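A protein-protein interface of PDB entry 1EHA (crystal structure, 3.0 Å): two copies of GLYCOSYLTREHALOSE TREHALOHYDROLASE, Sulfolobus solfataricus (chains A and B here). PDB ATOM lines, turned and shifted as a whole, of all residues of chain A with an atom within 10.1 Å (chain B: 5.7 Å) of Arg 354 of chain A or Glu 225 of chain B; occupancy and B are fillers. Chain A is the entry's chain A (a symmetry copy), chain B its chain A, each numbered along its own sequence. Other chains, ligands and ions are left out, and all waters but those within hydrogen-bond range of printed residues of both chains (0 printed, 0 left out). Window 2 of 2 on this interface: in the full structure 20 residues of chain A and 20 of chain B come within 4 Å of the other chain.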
ATOM      1  N   THR A 327      18.744 -12.284  21.855  1.00  0.00           N
ATOM      2  CA  THR A 327      18.798 -12.153  23.285  1.00  0.00           C
ATOM      3  C   THR A 327      19.287 -13.381  24.002  1.00  0.00           C
ATOM      4  O   THR A 327      19.806 -13.297  25.106  1.00  0.00           O
ATOM      5  CB  THR A 327      17.561 -11.573  23.978  1.00  0.00           C
ATOM      6  OG1 THR A 327      17.878 -11.456  25.343  1.00  0.00           O
ATOM      7  CG2 THR A 327      16.369 -12.488  23.821  1.00  0.00           C
ATOM      8  N   ASP A 328      19.147 -14.532  23.418  1.00  0.00           N
ATOM      9  CA  ASP A 328      19.630 -15.677  24.151  1.00  0.00           C
ATOM     10  C   ASP A 328      21.137 -15.777  24.123  1.00  0.00           C
ATOM     11  O   ASP A 328      21.750 -16.474  24.938  1.00  0.00           O
ATOM     12  CB  ASP A 328      18.951 -17.011  23.783  1.00  0.00           C
ATOM     13  CG  ASP A 328      17.555 -17.133  24.321  1.00  0.00           C
ATOM     14  OD1 ASP A 328      17.184 -16.595  25.370  1.00  0.00           O
ATOM     15  OD2 ASP A 328      16.778 -17.830  23.504  1.00  0.00           O
ATOM     16  N   TYR A 345      21.923 -24.362  23.943  1.00  0.00           N
ATOM     17  CA  TYR A 345      20.824 -24.761  24.814  1.00  0.00           C
ATOM     18  C   TYR A 345      20.676 -26.274  24.767  1.00  0.00           C
ATOM     19  O   TYR A 345      20.095 -26.900  23.869  1.00  0.00           O
ATOM     20  CB  TYR A 345      19.518 -24.047  24.590  1.00  0.00           C
ATOM     21  CG  TYR A 345      19.716 -22.603  24.879  1.00  0.00           C
ATOM     22  CD1 TYR A 345      20.677 -21.877  24.177  1.00  0.00           C
ATOM     23  CD2 TYR A 345      18.984 -21.968  25.875  1.00  0.00           C
ATOM     24  CE1 TYR A 345      20.890 -20.530  24.443  1.00  0.00           C
ATOM     25  CE2 TYR A 345      19.167 -20.610  26.142  1.00  0.00           C
ATOM     26  CZ  TYR A 345      20.121 -19.896  25.423  1.00  0.00           C
ATOM     27  OH  TYR A 345      20.296 -18.570  25.698  1.00  0.00           O
ATOM     28  N   LYS A 348      18.513 -25.686  29.201  1.00  0.00           N
ATOM     29  CA  LYS A 348      18.740 -24.530  30.068  1.00  0.00           C
ATOM     30  C   LYS A 348      17.766 -23.470  29.715  1.00  0.00           C
ATOM     31  O   LYS A 348      17.065 -23.602  28.692  1.00  0.00           O
ATOM     32  CB  LYS A 348      20.165 -23.997  30.134  1.00  0.00           C
ATOM     33  CG  LYS A 348      20.594 -23.167  28.918  1.00  0.00           C
ATOM     34  CD  LYS A 348      21.368 -23.976  27.881  1.00  0.00           C
ATOM     35  CE  LYS A 348      22.678 -24.549  28.422  1.00  0.00           C
ATOM     36  NZ  LYS A 348      22.644 -26.007  28.697  1.00  0.00           N
ATOM     37  N   TYR A 349      17.725 -22.436  30.550  1.00  0.00           N
ATOM     38  CA  TYR A 349      16.741 -21.391  30.375  1.00  0.00           C
ATOM     39  C   TYR A 349      16.855 -20.306  29.275  1.00  0.00           C
ATOM     40  O   TYR A 349      17.540 -19.308  29.403  1.00  0.00           O
ATOM     41  CB  TYR A 349      16.284 -20.839  31.742  1.00  0.00           C
ATOM     42  CG  TYR A 349      14.896 -20.240  31.762  1.00  0.00           C
ATOM     43  CD1 TYR A 349      14.452 -19.357  30.779  1.00  0.00           C
ATOM     44  CD2 TYR A 349      14.050 -20.512  32.832  1.00  0.00           C
ATOM     45  CE1 TYR A 349      13.176 -18.802  30.845  1.00  0.00           C
ATOM     46  CE2 TYR A 349      12.770 -19.970  32.915  1.00  0.00           C
ATOM     47  CZ  TYR A 349      12.337 -19.113  31.912  1.00  0.00           C
ATOM     48  OH  TYR A 349      11.110 -18.544  31.998  1.00  0.00           O
ATOM     49  N   SER A 350      16.052 -20.430  28.258  1.00  0.00           N
ATOM     50  CA  SER A 350      15.942 -19.423  27.272  1.00  0.00           C
ATOM     51  C   SER A 350      15.003 -18.318  27.762  1.00  0.00           C
ATOM     52  O   SER A 350      13.784 -18.469  27.767  1.00  0.00           O
ATOM     53  CB  SER A 350      15.311 -19.949  25.970  1.00  0.00           C
ATOM     54  OG  SER A 350      14.260 -19.058  25.528  1.00  0.00           O
ATOM     55  N   ASN A 351      15.506 -17.130  28.034  1.00  0.00           N
ATOM     56  CA  ASN A 351      14.578 -16.054  28.400  1.00  0.00           C
ATOM     57  C   ASN A 351      13.785 -15.698  27.217  1.00  0.00           C
ATOM     58  O   ASN A 351      12.865 -14.900  27.285  1.00  0.00           O
ATOM     59  CB  ASN A 351      15.299 -14.760  28.752  1.00  0.00           C
ATOM     60  CG  ASN A 351      16.362 -14.987  29.782  1.00  0.00           C
ATOM     61  OD1 ASN A 351      16.199 -14.575  30.945  1.00  0.00           O
ATOM     62  ND2 ASN A 351      17.413 -15.706  29.374  1.00  0.00           N
ATOM     63  N   PHE A 352      14.242 -16.215  26.103  1.00  0.00           N
ATOM     64  CA  PHE A 352      13.641 -15.919  24.870  1.00  0.00           C
ATOM     65  C   PHE A 352      12.306 -16.591  24.732  1.00  0.00           C
ATOM     66  O   PHE A 352      11.339 -16.005  24.208  1.00  0.00           O
ATOM     67  CB  PHE A 352      14.606 -16.086  23.686  1.00  0.00           C
ATOM     68  CG  PHE A 352      13.885 -15.911  22.393  1.00  0.00           C
ATOM     69  CD1 PHE A 352      13.008 -14.837  22.225  1.00  0.00           C
ATOM     70  CD2 PHE A 352      14.010 -16.860  21.381  1.00  0.00           C
ATOM     71  CE1 PHE A 352      12.234 -14.733  21.067  1.00  0.00           C
ATOM     72  CE2 PHE A 352      13.250 -16.761  20.216  1.00  0.00           C
ATOM     73  CZ  PHE A 352      12.381 -15.674  20.048  1.00  0.00           C
ATOM     74  N   ARG A 353      12.245 -17.800  25.272  1.00  0.00           N
ATOM     75  CA  ARG A 353      11.015 -18.562  25.244  1.00  0.00           C
ATOM     76  C   ARG A 353      10.539 -18.846  26.624  1.00  0.00           C
ATOM     77  O   ARG A 353       9.572 -19.569  26.825  1.00  0.00           O
ATOM     78  CB  ARG A 353      11.190 -19.827  24.466  1.00  0.00           C
ATOM     79  CG  ARG A 353      12.379 -19.634  23.568  1.00  0.00           C
ATOM     80  CD  ARG A 353      13.317 -20.811  23.559  1.00  0.00           C
ATOM     81  NE  ARG A 353      13.176 -21.421  22.256  1.00  0.00           N
ATOM     82  CZ  ARG A 353      14.045 -21.336  21.270  1.00  0.00           C
ATOM     83  NH1 ARG A 353      15.235 -20.720  21.380  1.00  0.00           N
ATOM     84  NH2 ARG A 353      13.713 -21.923  20.140  1.00  0.00           N
ATOM     85  N   ARG A 354      11.227 -18.222  27.572  1.00  0.00           N
ATOM     86  CA  ARG A 354      10.881 -18.370  28.962  1.00  0.00           C
ATOM     87  C   ARG A 354      10.596 -19.864  29.282  1.00  0.00           C
ATOM     88  O   ARG A 354       9.613 -20.307  29.926  1.00  0.00           O
ATOM     89  CB  ARG A 354       9.732 -17.422  29.271  1.00  0.00           C
ATOM     90  CG  ARG A 354       9.317 -16.545  28.083  1.00  0.00           C
ATOM     91  CD  ARG A 354       9.470 -15.062  28.389  1.00  0.00           C
ATOM     92  NE  ARG A 354      10.589 -14.823  29.303  1.00  0.00           N
ATOM     93  CZ  ARG A 354      10.482 -14.727  30.639  1.00  0.00           C
ATOM     94  NH1 ARG A 354       9.308 -14.814  31.269  1.00  0.00           N
ATOM     95  NH2 ARG A 354      11.585 -14.530  31.372  1.00  0.00           N
ATOM     96  N   LYS A 355      11.495 -20.666  28.793  1.00  0.00           N
ATOM     97  CA  LYS A 355      11.320 -22.054  28.923  1.00  0.00           C
ATOM     98  C   LYS A 355      12.656 -22.693  29.175  1.00  0.00           C
ATOM     99  O   LYS A 355      13.641 -21.983  29.359  1.00  0.00           O
ATOM    100  CB  LYS A 355      10.699 -22.498  27.592  1.00  0.00           C
ATOM    101  CG  LYS A 355      10.691 -23.987  27.305  1.00  0.00           C
ATOM    102  CD  LYS A 355      10.020 -24.292  26.004  1.00  0.00           C
ATOM    103  CE  LYS A 355      10.805 -25.284  25.170  1.00  0.00           C
ATOM    104  NZ  LYS A 355      10.845 -24.898  23.748  1.00  0.00           N
ATOM    105  N   THR A 356      12.666 -24.015  29.254  1.00  0.00           N
ATOM    106  CA  THR A 356      13.870 -24.770  29.406  1.00  0.00           C
ATOM    107  C   THR A 356      14.088 -25.484  28.098  1.00  0.00           C
ATOM    108  O   THR A 356      13.489 -26.530  27.819  1.00  0.00           O
ATOM    109  CB  THR A 356      13.960 -25.712  30.642  1.00  0.00           C
ATOM    110  OG1 THR A 356      14.039 -24.947  31.832  1.00  0.00           O
ATOM    111  CG2 THR A 356      15.208 -26.614  30.544  1.00  0.00           C
ATOM    112  N   HIS A 357      14.909 -24.859  27.271  1.00  0.00           N
ATOM    113  CA  HIS A 357      15.180 -25.353  25.950  1.00  0.00           C
ATOM    114  C   HIS A 357      16.299 -26.370  25.843  1.00  0.00           C
ATOM    115  O   HIS A 357      17.173 -26.456  26.680  1.00  0.00           O
ATOM    116  CB  HIS A 357      15.333 -24.193  24.966  1.00  0.00           C
ATOM    117  CG  HIS A 357      15.066 -24.580  23.581  1.00  0.00           C
ATOM    118  ND1 HIS A 357      15.666 -25.688  23.024  1.00  0.00           N
ATOM    119  CD2 HIS A 357      14.295 -24.004  22.658  1.00  0.00           C
ATOM    120  CE1 HIS A 357      15.232 -25.792  21.777  1.00  0.00           C
ATOM    121  NE2 HIS A 357      14.410 -24.787  21.524  1.00  0.00           N
ATOM    122  N   TRP B  16       2.022 -18.150  41.505  1.00  0.00           N
ATOM    123  CA  TRP B  16       2.296 -18.033  40.090  1.00  0.00           C
ATOM    124  C   TRP B  16       1.313 -17.086  39.433  1.00  0.00           C
ATOM    125  O   TRP B  16       0.173 -17.444  39.192  1.00  0.00           O
ATOM    126  CB  TRP B  16       2.086 -19.446  39.515  1.00  0.00           C
ATOM    127  CG  TRP B  16       2.415 -19.625  38.079  1.00  0.00           C
ATOM    128  CD1 TRP B  16       1.985 -20.616  37.252  1.00  0.00           C
ATOM    129  CD2 TRP B  16       3.286 -18.839  37.331  1.00  0.00           C
ATOM    130  NE1 TRP B  16       2.535 -20.473  36.009  1.00  0.00           N
ATOM    131  CE2 TRP B  16       3.337 -19.387  36.044  1.00  0.00           C
ATOM    132  CE3 TRP B  16       3.994 -17.712  37.640  1.00  0.00           C
ATOM    133  CZ2 TRP B  16       4.078 -18.818  35.069  1.00  0.00           C
ATOM    134  CZ3 TRP B  16       4.744 -17.140  36.674  1.00  0.00           C
ATOM    135  CH2 TRP B  16       4.782 -17.689  35.401  1.00  0.00           C
ATOM    136  N   PRO B  18       2.191 -14.652  36.589  1.00  0.00           N
ATOM    137  CA  PRO B  18       2.757 -13.945  35.487  1.00  0.00           C
ATOM    138  C   PRO B  18       1.908 -12.757  35.061  1.00  0.00           C
ATOM    139  O   PRO B  18       2.353 -11.610  35.125  1.00  0.00           O
ATOM    140  CB  PRO B  18       2.812 -14.936  34.330  1.00  0.00           C
ATOM    141  CG  PRO B  18       2.218 -16.248  34.814  1.00  0.00           C
ATOM    142  CD  PRO B  18       1.893 -16.065  36.277  1.00  0.00           C
ATOM    143  N   GLU B  39      10.165 -11.559  39.168  1.00  0.00           N
ATOM    144  CA  GLU B  39      10.228 -11.443  37.717  1.00  0.00           C
ATOM    145  C   GLU B  39       9.587 -12.624  36.977  1.00  0.00           C
ATOM    146  O   GLU B  39       8.897 -12.441  35.957  1.00  0.00           O
ATOM    147  CB  GLU B  39      11.669 -11.191  37.222  1.00  0.00           C
ATOM    148  CG  GLU B  39      12.724 -12.001  38.006  1.00  0.00           C
ATOM    149  CD  GLU B  39      12.984 -13.381  37.445  1.00  0.00           C
ATOM    150  OE1 GLU B  39      12.659 -13.729  36.301  1.00  0.00           O
ATOM    151  OE2 GLU B  39      13.629 -14.154  38.308  1.00  0.00           O
ATOM    152  N   LYS B  40       9.836 -13.848  37.478  1.00  0.00           N
ATOM    153  CA  LYS B  40       9.282 -15.032  36.836  1.00  0.00           C
ATOM    154  C   LYS B  40       7.786 -14.977  36.794  1.00  0.00           C
ATOM    155  O   LYS B  40       7.190 -15.590  35.935  1.00  0.00           O
ATOM    156  CB  LYS B  40       9.851 -16.376  37.268  1.00  0.00           C
ATOM    157  CG  LYS B  40      11.113 -16.782  36.479  1.00  0.00           C
ATOM    158  CD  LYS B  40      11.665 -18.199  36.771  1.00  0.00           C
ATOM    159  CE  LYS B  40      13.151 -18.236  37.190  1.00  0.00           C
ATOM    160  NZ  LYS B  40      13.378 -18.740  38.570  1.00  0.00           N
ATOM    161  N   PRO B 205      -0.744 -18.404  32.042  1.00  0.00           N
ATOM    162  CA  PRO B 205      -0.969 -19.470  31.110  1.00  0.00           C
ATOM    163  C   PRO B 205      -0.700 -20.780  31.752  1.00  0.00           C
ATOM    164  O   PRO B 205       0.443 -21.153  31.971  1.00  0.00           O
ATOM    165  CB  PRO B 205       0.095 -19.291  30.040  1.00  0.00           C
ATOM    166  CG  PRO B 205       1.228 -18.592  30.750  1.00  0.00           C
ATOM    167  CD  PRO B 205       0.686 -18.080  32.081  1.00  0.00           C
ATOM    168  N   ASN B 220      -0.335 -26.460  29.599  1.00  0.00           N
ATOM    169  CA  ASN B 220       0.790 -26.099  28.799  1.00  0.00           C
ATOM    170  C   ASN B 220       2.078 -26.704  29.305  1.00  0.00           C
ATOM    171  O   ASN B 220       2.640 -26.217  30.255  1.00  0.00           O
ATOM    172  CB  ASN B 220       0.917 -24.577  28.746  1.00  0.00           C
ATOM    173  CG  ASN B 220       2.012 -24.220  27.818  1.00  0.00           C
ATOM    174  OD1 ASN B 220       2.105 -24.814  26.724  1.00  0.00           O
ATOM    175  ND2 ASN B 220       2.943 -23.424  28.328  1.00  0.00           N
ATOM    176  N   ASP B 223       4.995 -24.883  25.418  1.00  0.00           N
ATOM    177  CA  ASP B 223       5.262 -23.475  25.139  1.00  0.00           C
ATOM    178  C   ASP B 223       5.813 -22.620  26.236  1.00  0.00           C
ATOM    179  O   ASP B 223       6.525 -23.067  27.128  1.00  0.00           O
ATOM    180  CB  ASP B 223       4.057 -22.751  24.510  1.00  0.00           C
ATOM    181  CG  ASP B 223       4.306 -22.336  23.093  1.00  0.00           C
ATOM    182  OD1 ASP B 223       5.225 -22.785  22.407  1.00  0.00           O
ATOM    183  OD2 ASP B 223       3.436 -21.444  22.684  1.00  0.00           O
ATOM    184  N   ALA B 224       5.453 -21.345  26.070  1.00  0.00           N
ATOM    185  CA  ALA B 224       5.827 -20.243  26.901  1.00  0.00           C
ATOM    186  C   ALA B 224       6.340 -20.608  28.287  1.00  0.00           C
ATOM    187  O   ALA B 224       7.543 -20.856  28.456  1.00  0.00           O
ATOM    188  CB  ALA B 224       4.752 -19.189  26.922  1.00  0.00           C
ATOM    189  N   GLU B 225       5.490 -20.628  29.308  1.00  0.00           N
ATOM    190  CA  GLU B 225       6.118 -20.931  30.585  1.00  0.00           C
ATOM    191  C   GLU B 225       6.109 -22.395  31.147  1.00  0.00           C
ATOM    192  O   GLU B 225       6.483 -22.619  32.315  1.00  0.00           O
ATOM    193  CB  GLU B 225       5.967 -19.796  31.624  1.00  0.00           C
ATOM    194  CG  GLU B 225       6.848 -18.551  31.341  1.00  0.00           C
ATOM    195  CD  GLU B 225       6.118 -17.220  31.441  1.00  0.00           C
ATOM    196  OE1 GLU B 225       5.292 -16.821  30.608  1.00  0.00           O
ATOM    197  OE2 GLU B 225       6.493 -16.515  32.492  1.00  0.00           O
ATOM    198  N   SER B 226       5.699 -23.375  30.308  1.00  0.00           N
ATOM    199  CA  SER B 226       5.613 -24.807  30.666  1.00  0.00           C
ATOM    200  C   SER B 226       6.308 -25.187  31.984  1.00  0.00           C
ATOM    201  O   SER B 226       5.835 -25.978  32.825  1.00  0.00           O
ATOM    202  CB  SER B 226       6.154 -25.661  29.544  1.00  0.00           C
ATOM    203  OG  SER B 226       7.473 -25.241  29.257  1.00  0.00           O
ATOM    204  N   ASP B 227       7.475 -24.649  32.085  1.00  0.00           N
ATOM    205  CA  ASP B 227       8.327 -24.779  33.196  1.00  0.00           C
ATOM    206  C   ASP B 227       7.564 -24.864  34.523  1.00  0.00           C
ATOM    207  O   ASP B 227       7.774 -25.801  35.302  1.00  0.00           O
ATOM    208  CB  ASP B 227       9.261 -23.539  33.175  1.00  0.00           C
ATOM    209  CG  ASP B 227      10.602 -23.832  32.566  1.00  0.00           C
ATOM    210  OD1 ASP B 227      11.654 -23.770  33.193  1.00  0.00           O
ATOM    211  OD2 ASP B 227      10.513 -24.228  31.325  1.00  0.00           O
ATOM    212  N   GLU B 228       6.742 -23.829  34.787  1.00  0.00           N
ATOM    213  CA  GLU B 228       5.956 -23.680  36.012  1.00  0.00           C
ATOM    214  C   GLU B 228       4.852 -24.737  36.119  1.00  0.00           C
ATOM    215  O   GLU B 228       4.878 -25.606  37.007  1.00  0.00           O
ATOM    216  CB  GLU B 228       5.347 -22.262  36.103  1.00  0.00           C
ATOM    217  CG  GLU B 228       6.382 -21.132  36.330  1.00  0.00           C
ATOM    218  CD  GLU B 228       7.830 -21.530  36.092  1.00  0.00           C
ATOM    219  OE1 GLU B 228       8.479 -21.203  35.086  1.00  0.00           O
ATOM    220  OE2 GLU B 228       8.347 -22.159  37.122  1.00  0.00           O
ATOM    221  N   VAL B 229       3.872 -24.654  35.204  1.00  0.00           N
ATOM    222  CA  VAL B 229       2.797 -25.611  35.169  1.00  0.00           C
ATOM    223  C   VAL B 229       3.318 -27.048  35.241  1.00  0.00           C
ATOM    224  O   VAL B 229       2.833 -27.912  35.968  1.00  0.00           O
ATOM    225  CB  VAL B 229       1.907 -25.423  33.950  1.00  0.00           C
ATOM    226  CG1 VAL B 229       2.151 -24.082  33.293  1.00  0.00           C
ATOM    227  CG2 VAL B 229       2.125 -26.541  32.966  1.00  0.00           C
ATOM    228  N   ARG B 230       4.330 -27.327  34.484  1.00  0.00           N
ATOM    229  CA  ARG B 230       4.838 -28.664  34.545  1.00  0.00           C
ATOM    230  C   ARG B 230       5.304 -29.022  35.985  1.00  0.00           C
ATOM    231  O   ARG B 230       5.388 -30.191  36.394  1.00  0.00           O
ATOM    232  CB  ARG B 230       5.847 -28.900  33.402  1.00  0.00           C
ATOM    233  CG  ARG B 230       7.306 -28.883  33.798  1.00  0.00           C
ATOM    234  CD  ARG B 230       8.076 -29.836  32.906  1.00  0.00           C
ATOM    235  NE  ARG B 230       7.394 -30.002  31.614  1.00  0.00           N
ATOM    236  CZ  ARG B 230       7.620 -31.026  30.757  1.00  0.00           C
ATOM    237  NH1 ARG B 230       8.472 -32.040  31.007  1.00  0.00           N
ATOM    238  NH2 ARG B 230       6.937 -31.032  29.614  1.00  0.00           N
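OD1 of Asp 227 of chain B touches CE2 of Tyr 349 of chain A, at 3.97 Å.
O of Asp 223 of chain B touches CD of Lys 355 of chain A, at 3.9 Å.
O of Ala 224 of chain B touches CB of Lys 355 of chain A, 3.7 Å away.
OG of Ser 226 of chain B touches CG of Lys 355 of chain A, 3.97 Å away.
Lys 355 of chain A touches Asp 227 of chain B (CA to OD2, 3.3 Å).
NH1 of Arg 353 of chain A is in salt-bridge range of OD2 of Asp 328 of chain A (3.9 Å).
O of Asp 223 of chain B lies within hydrogen-bond range of OG of Ser 226 of chain B, at 3.2 Å.
The backbone carbonyl oxygen (O) of Arg 354 of chain A sits close to the side-chain hydroxyl (OH) of Tyr 349 of chain A.
A ring nitrogen (NE2) of His 357 of chain A sits at hydrogen-bond distance from the guanidinium group (NH2) of Arg 353 of chain A (3.3 Å).
N of Ser 350 of chain A lies within hydrogen-bond range of O of Lys 355 of chain A, 3.1 Å away.
The side-chain amide nitrogen (ND2) of Asn 220 of chain B sits close to the backbone NH (N) of Ser 226 of chain B (3.4 Å).
Hydrophobic or aromatic side chains of chain A within 4 Å of the printed part of chain B: Tyr 349.
Printed residues of chain B that touch a printed residue of chain A: Asp 223, Ala 224, Glu 225, Ser 226 and Asp 227.
Of the printed residues of chain B, Tyr 349 of chain A touches Asp 227 (3.97 Å).
Of the printed residues of chain B, Arg 353 of chain A touches Ala 224.
Arg 354 of chain A touches two residues of chain B.
Of the printed residues of chain B, Lys 355 of chain A touches Asp 223, Ala 224, Ser 226 and Asp 227.
Pro 18 of chain B touches none of the printed residues of chain A.
Of the printed residues of chain A, Asp 223 of chain B touches Lys 355.
Of the printed residues of chain A, Ala 224 of chain B touches Arg 353 (2.9 Å), Arg 354 (2.6 Å) and Lys 355 (3.7 Å).
Glu 225 of chain B touches just one residue of chain A: Arg 354.
Of the printed residues of chain A, Ser 226 of chain B touches Lys 355 (3.97 Å).
No residue of chain A comes within 4 Å of Glu 228 of chain B.
The nearest residue of chain B that does not touch Arg 354 of chain A is Asp 227 of chain B (4.3 Å).
The nearest residue of chain A that does not touch Glu 225 of chain B is Tyr 349 of chain A (4.3 Å).
The side-chain carboxylate of Asp 227 of chain B sits at hydrogen-bond distance from the side-chain hydroxyl of Thr 356 of chain A, 3.0 Å away.
The backbone carbonyl oxygen (O) of Arg 354 of chain A lies close to the backbone carbonyl oxygen (O) of Ala 224 of chain B, 2.6 Å away.
The backbone carbonyl oxygen (O) of Ala 224 of chain B sits close to the backbone carbonyl oxygen (O) of Arg 353 of chain A.
OE2 of Glu 225 of chain B lies within salt-bridge range of NH1 of Arg 354 of chain A (3.5 Å).
No position is printed for both chains.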
